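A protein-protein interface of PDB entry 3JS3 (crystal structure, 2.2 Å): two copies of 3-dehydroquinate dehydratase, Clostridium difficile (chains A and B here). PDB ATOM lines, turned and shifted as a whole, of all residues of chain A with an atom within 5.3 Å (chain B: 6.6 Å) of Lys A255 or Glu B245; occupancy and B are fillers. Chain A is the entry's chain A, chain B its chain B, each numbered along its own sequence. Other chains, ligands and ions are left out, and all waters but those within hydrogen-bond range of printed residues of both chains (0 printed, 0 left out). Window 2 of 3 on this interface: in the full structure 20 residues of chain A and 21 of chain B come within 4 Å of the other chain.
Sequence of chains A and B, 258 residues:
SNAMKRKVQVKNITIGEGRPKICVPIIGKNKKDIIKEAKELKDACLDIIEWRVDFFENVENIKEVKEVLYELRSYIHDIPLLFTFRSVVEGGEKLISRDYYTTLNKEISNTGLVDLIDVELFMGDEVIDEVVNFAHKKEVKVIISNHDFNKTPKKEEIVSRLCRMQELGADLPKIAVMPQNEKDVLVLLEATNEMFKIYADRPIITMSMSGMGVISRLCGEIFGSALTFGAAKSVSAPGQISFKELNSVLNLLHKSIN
Leu A252 touches Ile B241 (CD1 to CG2, 3.4 Å). Leu A252 touches Glu B245 (CD1 to OE1, 3.2 Å). CG2 of Val B249 touches CD2 of Leu A252 (3.9 Å). Leu A253 touches Leu B218.
No position is printed for both chains. Of the 5 pairs that touch across the chains among the printed residues, none has its exchanged pair printed and touching as well.
OG of Ser A256 lies within hydrogen-bond range of O of Leu A253, at 3.3 Å. OG of Ser B242 is in hydrogen-bond range of OE1 of Glu B245, at 2.8 Å. The backbone carbonyl oxygen (O) of Glu B245 sits at hydrogen-bond distance from the side-chain hydroxyl (OG) of Ser B248 (2.7 Å).
The side-chain amino group (NZ) of Lys A255 lies within salt-bridge range of the side-chain carboxylate (OE2) of Glu B245, at 3.8 Å.
Of chain B, only Glu B245 (3.8 Å) comes within 4 Å of Lys A255. Glu B245 touches two residues of chain A. Of the printed residues of chain B, Leu A253 touches Leu B218. Of the printed residues of chain A, Ile B241 touches Leu A252. Of the printed residues of chain A, Leu B218 touches Leu A253 (3.7 Å). Printed residues of chain A within 4 Å of Val B249: Leu A252. Of the printed residues of chain B, Leu A252 touches Ile B241 (3.4 Å), Glu B245 (3.2 Å) and Val B249 (3.9 Å). Ser B242 touches none of the printed residues of chain A. The nearest residue of chain B that does not touch Lys A255 is Ile B241 (6.0 Å). The nearest printed residue of chain A that does not touch Glu B245 is Asn A251 (7.6 Å).
Of the 11 printed residues of chain B, 4 touch a printed residue of chain A. Of the 6 printed residues of chain A, 3 touch a printed residue of chain B.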
ATOM      1  N   ASN A 251     -25.012  -5.144  10.672  1.00  0.00           N
ATOM      2  CA  ASN A 251     -23.853  -4.236  10.765  1.00  0.00           C
ATOM      3  C   ASN A 251     -24.268  -2.772  10.647  1.00  0.00           C
ATOM      4  O   ASN A 251     -23.750  -1.912  11.361  1.00  0.00           O
ATOM      5  CB  ASN A 251     -22.791  -4.529   9.685  1.00  0.00           C
ATOM      6  CG  ASN A 251     -22.005  -5.811   9.936  1.00  0.00           C
ATOM      7  OD1 ASN A 251     -22.020  -6.394  11.037  1.00  0.00           O
ATOM      8  ND2 ASN A 251     -21.287  -6.247   8.906  1.00  0.00           N
ATOM      9  N   LEU A 252     -25.179  -2.502   9.716  1.00  0.00           N
ATOM     10  CA  LEU A 252     -25.726  -1.179   9.516  1.00  0.00           C
ATOM     11  C   LEU A 252     -26.414  -0.691  10.784  1.00  0.00           C
ATOM     12  O   LEU A 252     -26.316   0.479  11.136  1.00  0.00           O
ATOM     13  CB  LEU A 252     -26.744  -1.214   8.387  1.00  0.00           C
ATOM     14  CG  LEU A 252     -27.556   0.059   8.173  1.00  0.00           C
ATOM     15  CD1 LEU A 252     -26.616   1.185   7.787  1.00  0.00           C
ATOM     16  CD2 LEU A 252     -28.598  -0.175   7.102  1.00  0.00           C
ATOM     17  N   LEU A 253     -27.123  -1.577  11.464  1.00  0.00           N
ATOM     18  CA  LEU A 253     -27.820  -1.185  12.700  1.00  0.00           C
ATOM     19  C   LEU A 253     -26.904  -1.132  13.926  1.00  0.00           C
ATOM     20  O   LEU A 253     -27.256  -0.523  14.938  1.00  0.00           O
ATOM     21  CB  LEU A 253     -28.984  -2.113  12.989  1.00  0.00           C
ATOM     22  CG  LEU A 253     -30.111  -2.202  11.954  1.00  0.00           C
ATOM     23  CD1 LEU A 253     -31.152  -3.159  12.490  1.00  0.00           C
ATOM     24  CD2 LEU A 253     -30.726  -0.849  11.656  1.00  0.00           C
ATOM     25  N   HIS A 254     -25.740  -1.778  13.845  1.00  0.00           N
ATOM     26  CA  HIS A 254     -24.819  -1.798  14.960  1.00  0.00           C
ATOM     27  C   HIS A 254     -24.189  -0.405  15.134  1.00  0.00           C
ATOM     28  O   HIS A 254     -23.930   0.040  16.252  1.00  0.00           O
ATOM     29  CB  HIS A 254     -23.767  -2.888  14.749  1.00  0.00           C
ATOM     30  CG  HIS A 254     -22.843  -3.057  15.903  1.00  0.00           C
ATOM     31  ND1 HIS A 254     -23.233  -3.660  17.079  1.00  0.00           N
ATOM     32  CD2 HIS A 254     -21.532  -2.728  16.057  1.00  0.00           C
ATOM     33  CE1 HIS A 254     -22.204  -3.683  17.916  1.00  0.00           C
ATOM     34  NE2 HIS A 254     -21.163  -3.123  17.320  1.00  0.00           N
ATOM     35  N   LYS A 255     -23.980   0.285  14.011  1.00  0.00           N
ATOM     36  CA  LYS A 255     -23.429   1.641  14.014  1.00  0.00           C
ATOM     37  C   LYS A 255     -24.494   2.770  13.934  1.00  0.00           C
ATOM     38  O   LYS A 255     -24.146   3.939  13.710  1.00  0.00           O
ATOM     39  CB  LYS A 255     -22.301   1.787  12.954  1.00  0.00           C
ATOM     40  CG  LYS A 255     -22.602   1.381  11.486  1.00  0.00           C
ATOM     41  CD  LYS A 255     -23.482   2.383  10.755  1.00  0.00           C
ATOM     42  CE  LYS A 255     -23.511   2.120   9.239  1.00  0.00           C
ATOM     43  NZ  LYS A 255     -22.184   2.301   8.578  1.00  0.00           N
ATOM     44  N   SER A 256     -25.770   2.435  14.155  1.00  0.00           N
ATOM     45  CA  SER A 256     -26.840   3.450  14.141  1.00  0.00           C
ATOM     46  C   SER A 256     -27.402   3.619  15.559  1.00  0.00           C
ATOM     47  O   SER A 256     -27.123   4.622  16.230  1.00  0.00           O
ATOM     48  CB  SER A 256     -27.979   3.089  13.171  1.00  0.00           C
ATOM     49  OG  SER A 256     -28.833   2.090  13.718  1.00  0.00           O
ATOM     50  N   LEU B 218     -36.874   1.718   8.247  1.00  0.00           N
ATOM     51  CA  LEU B 218     -36.656   0.597   7.387  1.00  0.00           C
ATOM     52  C   LEU B 218     -37.874  -0.274   7.057  1.00  0.00           C
ATOM     53  O   LEU B 218     -37.868  -0.944   6.020  1.00  0.00           O
ATOM     54  CB  LEU B 218     -35.632  -0.310   8.049  1.00  0.00           C
ATOM     55  CG  LEU B 218     -34.310   0.298   8.523  1.00  0.00           C
ATOM     56  CD1 LEU B 218     -33.476  -0.759   9.183  1.00  0.00           C
ATOM     57  CD2 LEU B 218     -33.531   0.922   7.392  1.00  0.00           C
ATOM     58  N   ILE B 241     -29.906   6.995   8.390  1.00  0.00           N
ATOM     59  CA  ILE B 241     -28.978   6.056   7.783  1.00  0.00           C
ATOM     60  C   ILE B 241     -28.593   6.644   6.424  1.00  0.00           C
ATOM     61  O   ILE B 241     -29.385   7.407   5.846  1.00  0.00           O
ATOM     62  CB  ILE B 241     -29.694   4.722   7.478  1.00  0.00           C
ATOM     63  CG1 ILE B 241     -30.304   4.130   8.727  1.00  0.00           C
ATOM     64  CG2 ILE B 241     -28.742   3.720   6.864  1.00  0.00           C
ATOM     65  CD1 ILE B 241     -31.093   2.911   8.438  1.00  0.00           C
ATOM     66  N   SER B 242     -27.423   6.271   5.889  1.00  0.00           N
ATOM     67  CA  SER B 242     -26.996   6.773   4.583  1.00  0.00           C
ATOM     68  C   SER B 242     -28.003   6.267   3.571  1.00  0.00           C
ATOM     69  O   SER B 242     -28.449   5.131   3.677  1.00  0.00           O
ATOM     70  CB  SER B 242     -25.627   6.238   4.178  1.00  0.00           C
ATOM     71  OG  SER B 242     -25.798   4.973   3.587  1.00  0.00           O
ATOM     72  N   PHE B 243     -28.321   7.067   2.565  1.00  0.00           N
ATOM     73  CA  PHE B 243     -29.359   6.680   1.631  1.00  0.00           C
ATOM     74  C   PHE B 243     -29.054   5.500   0.736  1.00  0.00           C
ATOM     75  O   PHE B 243     -29.988   4.793   0.363  1.00  0.00           O
ATOM     76  CB  PHE B 243     -29.861   7.872   0.796  1.00  0.00           C
ATOM     77  CG  PHE B 243     -28.998   8.216  -0.342  1.00  0.00           C
ATOM     78  CD1 PHE B 243     -29.240   7.659  -1.589  1.00  0.00           C
ATOM     79  CD2 PHE B 243     -27.949   9.100  -0.190  1.00  0.00           C
ATOM     80  CE1 PHE B 243     -28.432   7.974  -2.682  1.00  0.00           C
ATOM     81  CE2 PHE B 243     -27.130   9.429  -1.271  1.00  0.00           C
ATOM     82  CZ  PHE B 243     -27.377   8.864  -2.528  1.00  0.00           C
ATOM     83  N   LYS B 244     -27.789   5.261   0.393  1.00  0.00           N
ATOM     84  CA  LYS B 244     -27.462   4.112  -0.447  1.00  0.00           C
ATOM     85  C   LYS B 244     -27.745   2.817   0.330  1.00  0.00           C
ATOM     86  O   LYS B 244     -28.288   1.870  -0.211  1.00  0.00           O
ATOM     87  CB  LYS B 244     -26.006   4.147  -0.906  1.00  0.00           C
ATOM     88  CG  LYS B 244     -25.586   5.425  -1.646  1.00  0.00           C
ATOM     89  CD  LYS B 244     -24.137   5.326  -2.174  1.00  0.00           C
ATOM     90  CE  LYS B 244     -23.667   6.633  -2.793  1.00  0.00           C
ATOM     91  NZ  LYS B 244     -22.293   6.522  -3.426  1.00  0.00           N
ATOM     92  N   GLU B 245     -27.393   2.801   1.609  1.00  0.00           N
ATOM     93  CA  GLU B 245     -27.634   1.633   2.474  1.00  0.00           C
ATOM     94  C   GLU B 245     -29.140   1.382   2.660  1.00  0.00           C
ATOM     95  O   GLU B 245     -29.636   0.258   2.538  1.00  0.00           O
ATOM     96  CB  GLU B 245     -26.930   1.845   3.818  1.00  0.00           C
ATOM     97  CG  GLU B 245     -25.373   1.806   3.691  1.00  0.00           C
ATOM     98  CD  GLU B 245     -24.618   2.426   4.887  1.00  0.00           C
ATOM     99  OE1 GLU B 245     -25.244   3.171   5.681  1.00  0.00           O
ATOM    100  OE2 GLU B 245     -23.386   2.198   5.008  1.00  0.00           O
ATOM    101  N   LEU B 246     -29.857   2.466   2.916  1.00  0.00           N
ATOM    102  CA  LEU B 246     -31.294   2.443   3.110  1.00  0.00           C
ATOM    103  C   LEU B 246     -31.997   1.828   1.909  1.00  0.00           C
ATOM    104  O   LEU B 246     -32.926   1.044   2.050  1.00  0.00           O
ATOM    105  CB  LEU B 246     -31.761   3.885   3.305  1.00  0.00           C
ATOM    106  CG  LEU B 246     -33.196   4.248   3.627  1.00  0.00           C
ATOM    107  CD1 LEU B 246     -33.669   3.543   4.894  1.00  0.00           C
ATOM    108  CD2 LEU B 246     -33.280   5.783   3.779  1.00  0.00           C
ATOM    109  N   ASN B 247     -31.536   2.180   0.724  1.00  0.00           N
ATOM    110  CA  ASN B 247     -32.146   1.684  -0.502  1.00  0.00           C
ATOM    111  C   ASN B 247     -32.065   0.161  -0.590  1.00  0.00           C
ATOM    112  O   ASN B 247     -33.057  -0.502  -0.901  1.00  0.00           O
ATOM    113  CB  ASN B 247     -31.510   2.404  -1.715  1.00  0.00           C
ATOM    114  CG  ASN B 247     -31.949   1.836  -3.049  1.00  0.00           C
ATOM    115  OD1 ASN B 247     -31.659   0.664  -3.379  1.00  0.00           O
ATOM    116  ND2 ASN B 247     -32.570   2.684  -3.875  1.00  0.00           N
ATOM    117  N   SER B 248     -30.900  -0.404  -0.298  1.00  0.00           N
ATOM    118  CA  SER B 248     -30.754  -1.846  -0.357  1.00  0.00           C
ATOM    119  C   SER B 248     -31.666  -2.574   0.665  1.00  0.00           C
ATOM    120  O   SER B 248     -32.293  -3.590   0.331  1.00  0.00           O
ATOM    121  CB  SER B 248     -29.291  -2.239  -0.178  1.00  0.00           C
ATOM    122  OG  SER B 248     -28.793  -1.770   1.053  1.00  0.00           O
ATOM    123  N   VAL B 249     -31.760  -2.050   1.885  1.00  0.00           N
ATOM    124  CA  VAL B 249     -32.609  -2.663   2.911  1.00  0.00           C
ATOM    125  C   VAL B 249     -34.101  -2.641   2.508  1.00  0.00           C
ATOM    126  O   VAL B 249     -34.809  -3.643   2.688  1.00  0.00           O
ATOM    127  CB  VAL B 249     -32.404  -2.023   4.278  1.00  0.00           C
ATOM    128  CG1 VAL B 249     -33.391  -2.580   5.270  1.00  0.00           C
ATOM    129  CG2 VAL B 249     -30.941  -2.261   4.775  1.00  0.00           C
ATOM    130  N   LEU B 250     -34.565  -1.518   1.950  1.00  0.00           N
ATOM    131  CA  LEU B 250     -35.951  -1.410   1.486  1.00  0.00           C
ATOM    132  C   LEU B 250     -36.204  -2.368   0.320  1.00  0.00           C
ATOM    133  O   LEU B 250     -37.246  -3.027   0.283  1.00  0.00           O
ATOM    134  CB  LEU B 250     -36.281   0.026   1.053  1.00  0.00           C
ATOM    135  CG  LEU B 250     -36.201   1.068   2.178  1.00  0.00           C
ATOM    136  CD1 LEU B 250     -36.534   2.446   1.657  1.00  0.00           C
ATOM    137  CD2 LEU B 250     -37.131   0.681   3.318  1.00  0.00           C
